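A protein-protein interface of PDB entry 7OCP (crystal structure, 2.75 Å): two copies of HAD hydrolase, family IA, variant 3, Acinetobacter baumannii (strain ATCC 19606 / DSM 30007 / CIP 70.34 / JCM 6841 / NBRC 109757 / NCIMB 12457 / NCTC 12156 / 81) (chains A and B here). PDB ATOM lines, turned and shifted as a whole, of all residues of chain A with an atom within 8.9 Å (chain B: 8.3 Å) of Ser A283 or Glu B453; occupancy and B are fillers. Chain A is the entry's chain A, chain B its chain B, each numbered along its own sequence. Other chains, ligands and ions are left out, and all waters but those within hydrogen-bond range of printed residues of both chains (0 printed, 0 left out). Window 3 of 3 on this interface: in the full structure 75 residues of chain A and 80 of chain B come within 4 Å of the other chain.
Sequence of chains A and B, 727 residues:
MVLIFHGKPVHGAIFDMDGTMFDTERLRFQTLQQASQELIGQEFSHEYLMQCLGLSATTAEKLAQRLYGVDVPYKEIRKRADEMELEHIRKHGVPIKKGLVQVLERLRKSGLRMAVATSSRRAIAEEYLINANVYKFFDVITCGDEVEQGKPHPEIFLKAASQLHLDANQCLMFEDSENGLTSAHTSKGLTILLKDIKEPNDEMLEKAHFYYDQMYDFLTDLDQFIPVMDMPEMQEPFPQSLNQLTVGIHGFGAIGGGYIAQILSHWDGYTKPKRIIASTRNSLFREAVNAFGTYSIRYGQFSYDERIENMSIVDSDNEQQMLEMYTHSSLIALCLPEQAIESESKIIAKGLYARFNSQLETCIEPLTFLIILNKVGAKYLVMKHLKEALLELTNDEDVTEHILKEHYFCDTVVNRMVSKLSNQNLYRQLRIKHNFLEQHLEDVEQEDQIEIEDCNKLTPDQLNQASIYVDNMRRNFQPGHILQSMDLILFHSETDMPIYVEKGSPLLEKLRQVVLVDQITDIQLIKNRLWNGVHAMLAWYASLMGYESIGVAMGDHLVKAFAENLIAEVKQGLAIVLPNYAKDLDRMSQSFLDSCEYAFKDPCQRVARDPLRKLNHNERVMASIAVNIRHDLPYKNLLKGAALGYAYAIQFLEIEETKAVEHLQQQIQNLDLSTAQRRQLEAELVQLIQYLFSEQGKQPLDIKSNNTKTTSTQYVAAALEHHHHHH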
ATOM      1  N   THR A 280      -9.239 -10.329 -16.352  1.00  0.00           N
ATOM      2  CA  THR A 280      -9.476  -9.578 -15.090  1.00  0.00           C
ATOM      3  C   THR A 280     -10.757 -10.093 -14.423  1.00  0.00           C
ATOM      4  O   THR A 280     -11.690 -10.483 -15.155  1.00  0.00           O
ATOM      5  CB  THR A 280      -9.537  -8.064 -15.341  1.00  0.00           C
ATOM      6  OG1 THR A 280      -9.746  -7.410 -14.088  1.00  0.00           O
ATOM      7  CG2 THR A 280     -10.629  -7.662 -16.309  1.00  0.00           C
ATOM      8  N   ARG A 281     -10.786 -10.089 -13.087  1.00  0.00           N
ATOM      9  CA  ARG A 281     -11.976 -10.431 -12.260  1.00  0.00           C
ATOM     10  C   ARG A 281     -12.866  -9.186 -12.140  1.00  0.00           C
ATOM     11  O   ARG A 281     -14.069  -9.349 -11.850  1.00  0.00           O
ATOM     12  CB  ARG A 281     -11.549 -10.938 -10.878  1.00  0.00           C
ATOM     13  CG  ARG A 281     -10.528 -12.069 -10.904  1.00  0.00           C
ATOM     14  CD  ARG A 281      -9.863 -12.273  -9.554  1.00  0.00           C
ATOM     15  NE  ARG A 281      -9.051 -11.129  -9.152  1.00  0.00           N
ATOM     16  CZ  ARG A 281      -8.533 -10.939  -7.938  1.00  0.00           C
ATOM     17  NH1 ARG A 281      -7.812  -9.856  -7.693  1.00  0.00           N
ATOM     18  NH2 ARG A 281      -8.735 -11.819  -6.972  1.00  0.00           N
ATOM     19  N   ASN A 282     -12.286  -7.998 -12.357  1.00  0.00           N
ATOM     20  CA  ASN A 282     -12.965  -6.674 -12.314  1.00  0.00           C
ATOM     21  C   ASN A 282     -13.967  -6.582 -13.474  1.00  0.00           C
ATOM     22  O   ASN A 282     -13.523  -6.411 -14.627  1.00  0.00           O
ATOM     23  CB  ASN A 282     -11.944  -5.531 -12.352  1.00  0.00           C
ATOM     24  CG  ASN A 282     -12.537  -4.173 -12.040  1.00  0.00           C
ATOM     25  OD1 ASN A 282     -13.657  -3.867 -12.440  1.00  0.00           O
ATOM     26  ND2 ASN A 282     -11.784  -3.344 -11.334  1.00  0.00           N
ATOM     27  N   SER A 283     -15.264  -6.680 -13.168  1.00  0.00           N
ATOM     28  CA  SER A 283     -16.386  -6.667 -14.145  1.00  0.00           C
ATOM     29  C   SER A 283     -16.517  -5.281 -14.790  1.00  0.00           C
ATOM     30  O   SER A 283     -16.728  -5.225 -16.017  1.00  0.00           O
ATOM     31  CB  SER A 283     -17.675  -7.089 -13.490  1.00  0.00           C
ATOM     32  OG  SER A 283     -17.925  -6.314 -12.326  1.00  0.00           O
ATOM     33  N   LEU A 284     -16.401  -4.214 -13.989  1.00  0.00           N
ATOM     34  CA  LEU A 284     -16.514  -2.797 -14.437  1.00  0.00           C
ATOM     35  C   LEU A 284     -15.479  -2.523 -15.535  1.00  0.00           C
ATOM     36  O   LEU A 284     -15.863  -1.945 -16.570  1.00  0.00           O
ATOM     37  CB  LEU A 284     -16.308  -1.867 -13.236  1.00  0.00           C
ATOM     38  CG  LEU A 284     -16.471  -0.372 -13.512  1.00  0.00           C
ATOM     39  CD1 LEU A 284     -17.895  -0.043 -13.932  1.00  0.00           C
ATOM     40  CD2 LEU A 284     -16.074   0.448 -12.295  1.00  0.00           C
ATOM     41  N   PHE A 285     -14.224  -2.927 -15.313  1.00  0.00           N
ATOM     42  CA  PHE A 285     -13.089  -2.760 -16.260  1.00  0.00           C
ATOM     43  C   PHE A 285     -13.372  -3.522 -17.561  1.00  0.00           C
ATOM     44  O   PHE A 285     -13.161  -2.944 -18.644  1.00  0.00           O
ATOM     45  CB  PHE A 285     -11.772  -3.219 -15.626  1.00  0.00           C
ATOM     46  CG  PHE A 285     -10.977  -2.119 -14.968  1.00  0.00           C
ATOM     47  CD1 PHE A 285     -11.468  -1.453 -13.857  1.00  0.00           C
ATOM     48  CD2 PHE A 285      -9.736  -1.748 -15.465  1.00  0.00           C
ATOM     49  CE1 PHE A 285     -10.735  -0.440 -13.255  1.00  0.00           C
ATOM     50  CE2 PHE A 285      -9.007  -0.734 -14.864  1.00  0.00           C
ATOM     51  CZ  PHE A 285      -9.507  -0.083 -13.761  1.00  0.00           C
ATOM     52  N   ARG A 286     -13.832  -4.774 -17.452  1.00  0.00           N
ATOM     53  CA  ARG A 286     -14.096  -5.681 -18.604  1.00  0.00           C
ATOM     54  C   ARG A 286     -15.181  -5.075 -19.501  1.00  0.00           C
ATOM     55  O   ARG A 286     -14.919  -4.904 -20.708  1.00  0.00           O
ATOM     56  CB  ARG A 286     -14.516  -7.074 -18.117  1.00  0.00           C
ATOM     57  CG  ARG A 286     -14.852  -8.049 -19.238  1.00  0.00           C
ATOM     58  CD  ARG A 286     -15.113  -9.464 -18.755  1.00  0.00           C
ATOM     59  NE  ARG A 286     -16.231  -9.543 -17.820  1.00  0.00           N
ATOM     60  CZ  ARG A 286     -16.130  -9.600 -16.492  1.00  0.00           C
ATOM     61  NH1 ARG A 286     -14.947  -9.589 -15.897  1.00  0.00           N
ATOM     62  NH2 ARG A 286     -17.226  -9.668 -15.757  1.00  0.00           N
ATOM     63  N   GLU A 287     -16.346  -4.764 -18.923  1.00  0.00           N
ATOM     64  CA  GLU A 287     -17.561  -4.312 -19.655  1.00  0.00           C
ATOM     65  C   GLU A 287     -17.323  -2.924 -20.264  1.00  0.00           C
ATOM     66  O   GLU A 287     -17.864  -2.670 -21.359  1.00  0.00           O
ATOM     67  CB  GLU A 287     -18.775  -4.304 -18.721  1.00  0.00           C
ATOM     68  CG  GLU A 287     -19.174  -5.684 -18.219  1.00  0.00           C
ATOM     69  CD  GLU A 287     -19.796  -6.611 -19.252  1.00  0.00           C
ATOM     70  OE1 GLU A 287     -20.044  -6.159 -20.388  1.00  0.00           O
ATOM     71  OE2 GLU A 287     -20.035  -7.789 -18.913  1.00  0.00           O
ATOM     72  N   ALA A 288     -16.545  -2.070 -19.590  1.00  0.00           N
ATOM     73  CA  ALA A 288     -16.242  -0.676 -20.002  1.00  0.00           C
ATOM     74  C   ALA A 288     -15.352  -0.674 -21.253  1.00  0.00           C
ATOM     75  O   ALA A 288     -15.666   0.071 -22.201  1.00  0.00           O
ATOM     76  CB  ALA A 288     -15.589   0.076 -18.869  1.00  0.00           C
ATOM     77  N   VAL A 289     -14.276  -1.466 -21.241  1.00  0.00           N
ATOM     78  CA  VAL A 289     -13.292  -1.568 -22.361  1.00  0.00           C
ATOM     79  C   VAL A 289     -13.995  -2.173 -23.582  1.00  0.00           C
ATOM     80  O   VAL A 289     -13.755  -1.678 -24.699  1.00  0.00           O
ATOM     81  CB  VAL A 289     -12.052  -2.391 -21.959  1.00  0.00           C
ATOM     82  CG1 VAL A 289     -11.184  -2.740 -23.159  1.00  0.00           C
ATOM     83  CG2 VAL A 289     -11.230  -1.679 -20.897  1.00  0.00           C
ATOM     84  N   ASN A 290     -14.824  -3.199 -23.370  1.00  0.00           N
ATOM     85  CA  ASN A 290     -15.536  -3.938 -24.448  1.00  0.00           C
ATOM     86  C   ASN A 290     -16.653  -3.057 -25.025  1.00  0.00           C
ATOM     87  O   ASN A 290     -16.997  -3.252 -26.207  1.00  0.00           O
ATOM     88  CB  ASN A 290     -16.061  -5.288 -23.951  1.00  0.00           C
ATOM     89  CG  ASN A 290     -14.953  -6.256 -23.592  1.00  0.00           C
ATOM     90  OD1 ASN A 290     -13.861  -6.201 -24.154  1.00  0.00           O
ATOM     91  ND2 ASN A 290     -15.223  -7.150 -22.655  1.00  0.00           N
ATOM     92  N   ALA A 291     -17.188  -2.125 -24.229  1.00  0.00           N
ATOM     93  CA  ALA A 291     -18.207  -1.135 -24.654  1.00  0.00           C
ATOM     94  C   ALA A 291     -17.566  -0.111 -25.599  1.00  0.00           C
ATOM     95  O   ALA A 291     -18.149   0.145 -26.668  1.00  0.00           O
ATOM     96  CB  ALA A 291     -18.826  -0.462 -23.453  1.00  0.00           C
ATOM     97  N   ILE A 313     -11.247  -7.881 -23.516  1.00  0.00           N
ATOM     98  CA  ILE A 313     -11.135  -8.215 -22.064  1.00  0.00           C
ATOM     99  C   ILE A 313     -12.091  -9.375 -21.762  1.00  0.00           C
ATOM    100  O   ILE A 313     -13.230  -9.350 -22.273  1.00  0.00           O
ATOM    101  CB  ILE A 313     -11.416  -6.990 -21.168  1.00  0.00           C
ATOM    102  CG1 ILE A 313     -10.668  -5.737 -21.635  1.00  0.00           C
ATOM    103  CG2 ILE A 313     -11.104  -7.313 -19.713  1.00  0.00           C
ATOM    104  CD1 ILE A 313      -9.166  -5.886 -21.674  1.00  0.00           C
ATOM    105  N   VAL A 314     -11.637 -10.346 -20.961  1.00  0.00           N
ATOM    106  CA  VAL A 314     -12.392 -11.583 -20.595  1.00  0.00           C
ATOM    107  C   VAL A 314     -12.338 -11.771 -19.074  1.00  0.00           C
ATOM    108  O   VAL A 314     -11.494 -11.122 -18.426  1.00  0.00           O
ATOM    109  CB  VAL A 314     -11.842 -12.821 -21.332  1.00  0.00           C
ATOM    110  CG1 VAL A 314     -12.023 -12.705 -22.838  1.00  0.00           C
ATOM    111  CG2 VAL A 314     -10.384 -13.098 -20.992  1.00  0.00           C
ATOM    112  N   ASP A 315     -13.212 -12.629 -18.538  1.00  0.00           N
ATOM    113  CA  ASP A 315     -13.280 -12.981 -17.094  1.00  0.00           C
ATOM    114  C   ASP A 315     -12.242 -14.072 -16.804  1.00  0.00           C
ATOM    115  O   ASP A 315     -12.169 -15.039 -17.590  1.00  0.00           O
ATOM    116  CB  ASP A 315     -14.693 -13.424 -16.701  1.00  0.00           C
ATOM    117  CG  ASP A 315     -14.911 -13.598 -15.206  1.00  0.00           C
ATOM    118  OD1 ASP A 315     -13.968 -13.332 -14.432  1.00  0.00           O
ATOM    119  OD2 ASP A 315     -16.029 -13.996 -14.824  1.00  0.00           O
ATOM    120  N   SER A 316     -11.475 -13.917 -15.719  1.00  0.00           N
ATOM    121  CA  SER A 316     -10.420 -14.863 -15.265  1.00  0.00           C
ATOM    122  C   SER A 316     -11.049 -16.188 -14.810  1.00  0.00           C
ATOM    123  O   SER A 316     -10.401 -17.237 -14.990  1.00  0.00           O
ATOM    124  CB  SER A 316      -9.582 -14.255 -14.170  1.00  0.00           C
ATOM    125  OG  SER A 316      -8.928 -13.080 -14.625  1.00  0.00           O
ATOM    126  N   ASP A 317     -12.257 -16.136 -14.240  1.00  0.00           N
ATOM    127  CA  ASP A 317     -12.993 -17.319 -13.720  1.00  0.00           C
ATOM    128  C   ASP A 317     -13.559 -18.138 -14.886  1.00  0.00           C
ATOM    129  O   ASP A 317     -13.683 -19.370 -14.730  1.00  0.00           O
ATOM    130  CB  ASP A 317     -14.100 -16.901 -12.749  1.00  0.00           C
ATOM    131  CG  ASP A 317     -13.588 -16.234 -11.483  1.00  0.00           C
ATOM    132  OD1 ASP A 317     -12.373 -15.958 -11.413  1.00  0.00           O
ATOM    133  OD2 ASP A 317     -14.409 -15.999 -10.575  1.00  0.00           O
ATOM    134  N   LYS A 420      -2.806   1.830 -11.704  1.00  0.00           N
ATOM    135  CA  LYS A 420      -4.150   1.406 -12.183  1.00  0.00           C
ATOM    136  C   LYS A 420      -5.204   2.330 -11.563  1.00  0.00           C
ATOM    137  O   LYS A 420      -5.136   2.564 -10.339  1.00  0.00           O
ATOM    138  CB  LYS A 420      -4.400  -0.061 -11.822  1.00  0.00           C
ATOM    139  CG  LYS A 420      -5.750  -0.625 -12.248  1.00  0.00           C
ATOM    140  CD  LYS A 420      -5.852  -2.126 -12.072  1.00  0.00           C
ATOM    141  CE  LYS A 420      -7.275  -2.638 -12.123  1.00  0.00           C
ATOM    142  NZ  LYS A 420      -7.323  -4.120 -12.127  1.00  0.00           N
ATOM    143  N   ASN A 423     -11.902   2.234  -9.093  1.00  0.00           N
ATOM    144  CA  ASN A 423     -13.281   1.995  -9.601  1.00  0.00           C
ATOM    145  C   ASN A 423     -14.143   3.236  -9.344  1.00  0.00           C
ATOM    146  O   ASN A 423     -15.053   3.498 -10.156  1.00  0.00           O
ATOM    147  CB  ASN A 423     -13.907   0.746  -8.976  1.00  0.00           C
ATOM    148  CG  ASN A 423     -13.179  -0.526  -9.352  1.00  0.00           C
ATOM    149  OD1 ASN A 423     -13.572  -1.216 -10.291  1.00  0.00           O
ATOM    150  ND2 ASN A 423     -12.110  -0.836  -8.636  1.00  0.00           N
ATOM    151  N   LEU A 426     -13.178   5.544 -12.094  1.00  0.00           N
ATOM    152  CA  LEU A 426     -13.672   4.963 -13.373  1.00  0.00           C
ATOM    153  C   LEU A 426     -15.160   5.296 -13.541  1.00  0.00           C
ATOM    154  O   LEU A 426     -15.527   5.808 -14.615  1.00  0.00           O
ATOM    155  CB  LEU A 426     -13.433   3.449 -13.383  1.00  0.00           C
ATOM    156  CG  LEU A 426     -13.889   2.712 -14.644  1.00  0.00           C
ATOM    157  CD1 LEU A 426     -13.409   3.417 -15.904  1.00  0.00           C
ATOM    158  CD2 LEU A 426     -13.408   1.270 -14.630  1.00  0.00           C
ATOM    159  N   LEU A 430     -16.922   7.481 -16.422  1.00  0.00           N
ATOM    160  CA  LEU A 430     -18.025   6.906 -17.245  1.00  0.00           C
ATOM    161  C   LEU A 430     -19.259   7.814 -17.178  1.00  0.00           C
ATOM    162  O   LEU A 430     -19.944   7.951 -18.209  1.00  0.00           O
ATOM    163  CB  LEU A 430     -18.357   5.494 -16.746  1.00  0.00           C
ATOM    164  CG  LEU A 430     -17.295   4.427 -17.014  1.00  0.00           C
ATOM    165  CD1 LEU A 430     -17.589   3.162 -16.222  1.00  0.00           C
ATOM    166  CD2 LEU A 430     -17.193   4.110 -18.498  1.00  0.00           C
ATOM    167  N   ILE B 450     -24.317  -8.260 -19.524  1.00  0.00           N
ATOM    168  CA  ILE B 450     -23.986  -6.801 -19.494  1.00  0.00           C
ATOM    169  C   ILE B 450     -23.964  -6.294 -18.043  1.00  0.00           C
ATOM    170  O   ILE B 450     -23.263  -5.293 -17.788  1.00  0.00           O
ATOM    171  CB  ILE B 450     -24.959  -5.989 -20.379  1.00  0.00           C
ATOM    172  CG1 ILE B 450     -24.463  -4.558 -20.611  1.00  0.00           C
ATOM    173  CG2 ILE B 450     -26.376  -6.001 -19.817  1.00  0.00           C
ATOM    174  CD1 ILE B 450     -23.076  -4.468 -21.209  1.00  0.00           C
ATOM    175  N   GLU B 451     -24.704  -6.947 -17.137  1.00  0.00           N
ATOM    176  CA  GLU B 451     -24.764  -6.615 -15.686  1.00  0.00           C
ATOM    177  C   GLU B 451     -23.347  -6.592 -15.099  1.00  0.00           C
ATOM    178  O   GLU B 451     -22.640  -7.613 -15.225  1.00  0.00           O
ATOM    179  CB  GLU B 451     -25.628  -7.632 -14.935  1.00  0.00           C
ATOM    180  CG  GLU B 451     -27.117  -7.499 -15.211  1.00  0.00           C
ATOM    181  CD  GLU B 451     -27.837  -6.425 -14.412  1.00  0.00           C
ATOM    182  OE1 GLU B 451     -27.163  -5.500 -13.914  1.00  0.00           O
ATOM    183  OE2 GLU B 451     -29.075  -6.519 -14.288  1.00  0.00           O
ATOM    184  N   ILE B 452     -22.956  -5.468 -14.487  1.00  0.00           N
ATOM    185  CA  ILE B 452     -21.654  -5.287 -13.777  1.00  0.00           C
ATOM    186  C   ILE B 452     -21.796  -5.886 -12.372  1.00  0.00           C
ATOM    187  O   ILE B 452     -22.276  -5.174 -11.468  1.00  0.00           O
ATOM    188  CB  ILE B 452     -21.242  -3.799 -13.753  1.00  0.00           C
ATOM    189  CG1 ILE B 452     -21.097  -3.236 -15.171  1.00  0.00           C
ATOM    190  CG2 ILE B 452     -19.972  -3.595 -12.938  1.00  0.00           C
ATOM    191  CD1 ILE B 452     -21.095  -1.727 -15.241  1.00  0.00           C
ATOM    192  N   GLU B 453     -21.400  -7.153 -12.210  1.00  0.00           N
ATOM    193  CA  GLU B 453     -21.631  -7.968 -10.986  1.00  0.00           C
ATOM    194  C   GLU B 453     -20.546  -7.679  -9.943  1.00  0.00           C
ATOM    195  O   GLU B 453     -19.490  -7.131 -10.319  1.00  0.00           O
ATOM    196  CB  GLU B 453     -21.649  -9.459 -11.331  1.00  0.00           C
ATOM    197  CG  GLU B 453     -22.849  -9.875 -12.164  1.00  0.00           C
ATOM    198  CD  GLU B 453     -22.907 -11.356 -12.498  1.00  0.00           C
ATOM    199  OE1 GLU B 453     -21.838 -11.946 -12.757  1.00  0.00           O
ATOM    200  OE2 GLU B 453     -24.021 -11.916 -12.496  1.00  0.00           O
ATOM    201  N   ASP B 454     -20.821  -8.039  -8.683  1.00  0.00           N
ATOM    202  CA  ASP B 454     -19.897  -7.960  -7.517  1.00  0.00           C
ATOM    203  C   ASP B 454     -19.688  -6.495  -7.112  1.00  0.00           C
ATOM    204  O   ASP B 454     -19.786  -5.608  -7.984  1.00  0.00           O
ATOM    205  CB  ASP B 454     -18.563  -8.657  -7.804  1.00  0.00           C
ATOM    206  CG  ASP B 454     -18.700 -10.126  -8.172  1.00  0.00           C
ATOM    207  OD1 ASP B 454     -19.482 -10.830  -7.501  1.00  0.00           O
ATOM    208  OD2 ASP B 454     -18.022 -10.555  -9.128  1.00  0.00           O
ATOM    209  N   CYS B 455     -19.414  -6.263  -5.824  1.00  0.00           N
ATOM    210  CA  CYS B 455     -19.083  -4.934  -5.244  1.00  0.00           C
ATOM    211  C   CYS B 455     -17.609  -4.617  -5.519  1.00  0.00           C
ATOM    212  O   CYS B 455     -16.742  -5.204  -4.840  1.00  0.00           O
ATOM    213  CB  CYS B 455     -19.362  -4.895  -3.745  1.00  0.00           C
ATOM    214  SG  CYS B 455     -18.825  -3.355  -2.954  1.00  0.00           S
ATOM    215  N   ASN B 456     -17.345  -3.724  -6.480  1.00  0.00           N
ATOM    216  CA  ASN B 456     -15.982  -3.263  -6.860  1.00  0.00           C
ATOM    217  C   ASN B 456     -15.644  -1.995  -6.063  1.00  0.00           C
ATOM    218  O   ASN B 456     -15.164  -1.022  -6.678  1.00  0.00           O
ATOM    219  CB  ASN B 456     -15.871  -3.027  -8.370  1.00  0.00           C
ATOM    220  CG  ASN B 456     -16.204  -4.251  -9.197  1.00  0.00           C
ATOM    221  OD1 ASN B 456     -17.043  -4.189 -10.094  1.00  0.00           O
ATOM    222  ND2 ASN B 456     -15.554  -5.366  -8.907  1.00  0.00           N
ATOM    223  N   LEU B 458     -17.831  -0.077  -4.751  1.00  0.00           N
ATOM    224  CA  LEU B 458     -18.899   0.870  -5.174  1.00  0.00           C
ATOM    225  C   LEU B 458     -20.225   0.442  -4.537  1.00  0.00           C
ATOM    226  O   LEU B 458     -20.394  -0.768  -4.284  1.00  0.00           O
ATOM    227  CB  LEU B 458     -19.005   0.868  -6.704  1.00  0.00           C
ATOM    228  CG  LEU B 458     -17.803   1.436  -7.457  1.00  0.00           C
ATOM    229  CD1 LEU B 458     -17.891   1.114  -8.941  1.00  0.00           C
ATOM    230  CD2 LEU B 458     -17.683   2.937  -7.245  1.00  0.00           C
ATOM    231  N   LEU B 463     -23.462   0.907  -8.868  1.00  0.00           N
ATOM    232  CA  LEU B 463     -23.247  -0.338  -9.656  1.00  0.00           C
ATOM    233  C   LEU B 463     -24.382  -0.511 -10.675  1.00  0.00           C
ATOM    234  O   LEU B 463     -24.090  -0.922 -11.816  1.00  0.00           O
ATOM    235  CB  LEU B 463     -23.177  -1.536  -8.702  1.00  0.00           C
ATOM    236  CG  LEU B 463     -22.422  -2.753  -9.234  1.00  0.00           C
ATOM    237  CD1 LEU B 463     -20.918  -2.529  -9.171  1.00  0.00           C
ATOM    238  CD2 LEU B 463     -22.805  -4.008  -8.467  1.00  0.00           C
ATOM    239  N   SER B 467     -24.163   0.084 -14.854  1.00  0.00           N
ATOM    240  CA  SER B 467     -24.724  -0.934 -15.783  1.00  0.00           C
ATOM    241  C   SER B 467     -25.535  -0.248 -16.890  1.00  0.00           C
ATOM    242  O   SER B 467     -25.424  -0.683 -18.052  1.00  0.00           O
ATOM    243  CB  SER B 467     -25.560  -1.948 -15.044  1.00  0.00           C
ATOM    244  OG  SER B 467     -24.764  -2.690 -14.131  1.00  0.00           O
ATOM    245  N   VAL B 470     -22.933   1.810 -19.231  1.00  0.00           N
ATOM    246  CA  VAL B 470     -22.081   0.900 -20.057  1.00  0.00           C
ATOM    247  C   VAL B 470     -22.943   0.228 -21.135  1.00  0.00           C
ATOM    248  O   VAL B 470     -22.488   0.179 -22.296  1.00  0.00           O
ATOM    249  CB  VAL B 470     -21.351  -0.135 -19.177  1.00  0.00           C
ATOM    250  CG1 VAL B 470     -20.686  -1.225 -20.003  1.00  0.00           C
ATOM    251  CG2 VAL B 470     -20.336   0.534 -18.261  1.00  0.00           C
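Among the printed residues, pairs that only touch across the chains: Ser A283 with Ile B452, Leu A284 with Ile B452, Leu A284 with Asn B456, Leu A284 with Leu B458, Glu A287 with Ile B450, Glu A287 with Val B470, Ala A291 with Val B470, Asn A423 with Asn B456 and Asn A423 with Leu B458.
Hydrophobic or aromatic side chains of chain B within 4 Å of the printed part of chain A: Ile B450, Ile B452, Leu B458 and Val B470.
Among the printed residues, no Asp or Glu carboxylate lies within 4 Å of a Lys or Arg side-chain nitrogen of the other chain.
Of chain B, only Ile B452 (3.5 Å), Glu B453 (2.7 Å) and Asn B456 (3.2 Å) come within 4 Å of Ser A283.
Of the printed residues of chain B, Glu A287 touches Ile B450 and Val B470.
Printed residues of chain B within 4 Å of Ala A291: Val B470.
Lys A420 touches none of the printed residues of chain B.
No residue of chain A comes within 4 Å of Asp B454.
Ser B467 touches none of the printed residues of chain A.
The nearest residue of chain A that does not touch Glu B453 is Leu A284 (5.6 Å).
The nearest printed residue of chain A that does not touch Asn B456 is Asn A282 (4.1 Å).
No position is printed for both chains.
O of Glu B453 sits at hydrogen-bond distance from OG of Ser A283, at 2.7 Å.
The side-chain hydroxyl (OG) of Ser A283 sits at hydrogen-bond distance from the side-chain amide oxygen (OD1) of Asn B456, 3.2 Å away.
N of Leu A284 lies within hydrogen-bond range of OD1 of Asn A282 (3.2 Å).
The side-chain amide nitrogen of Asn A282 sits at hydrogen-bond distance from the side-chain amide oxygen of Asn A423, 3.0 Å away.
The side-chain hydroxyl (OG) of Ser B467 sits at hydrogen-bond distance from the backbone NH (N) of Ile B452.
SG of Cys B455 sits at hydrogen-bond distance from O of Leu B458.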
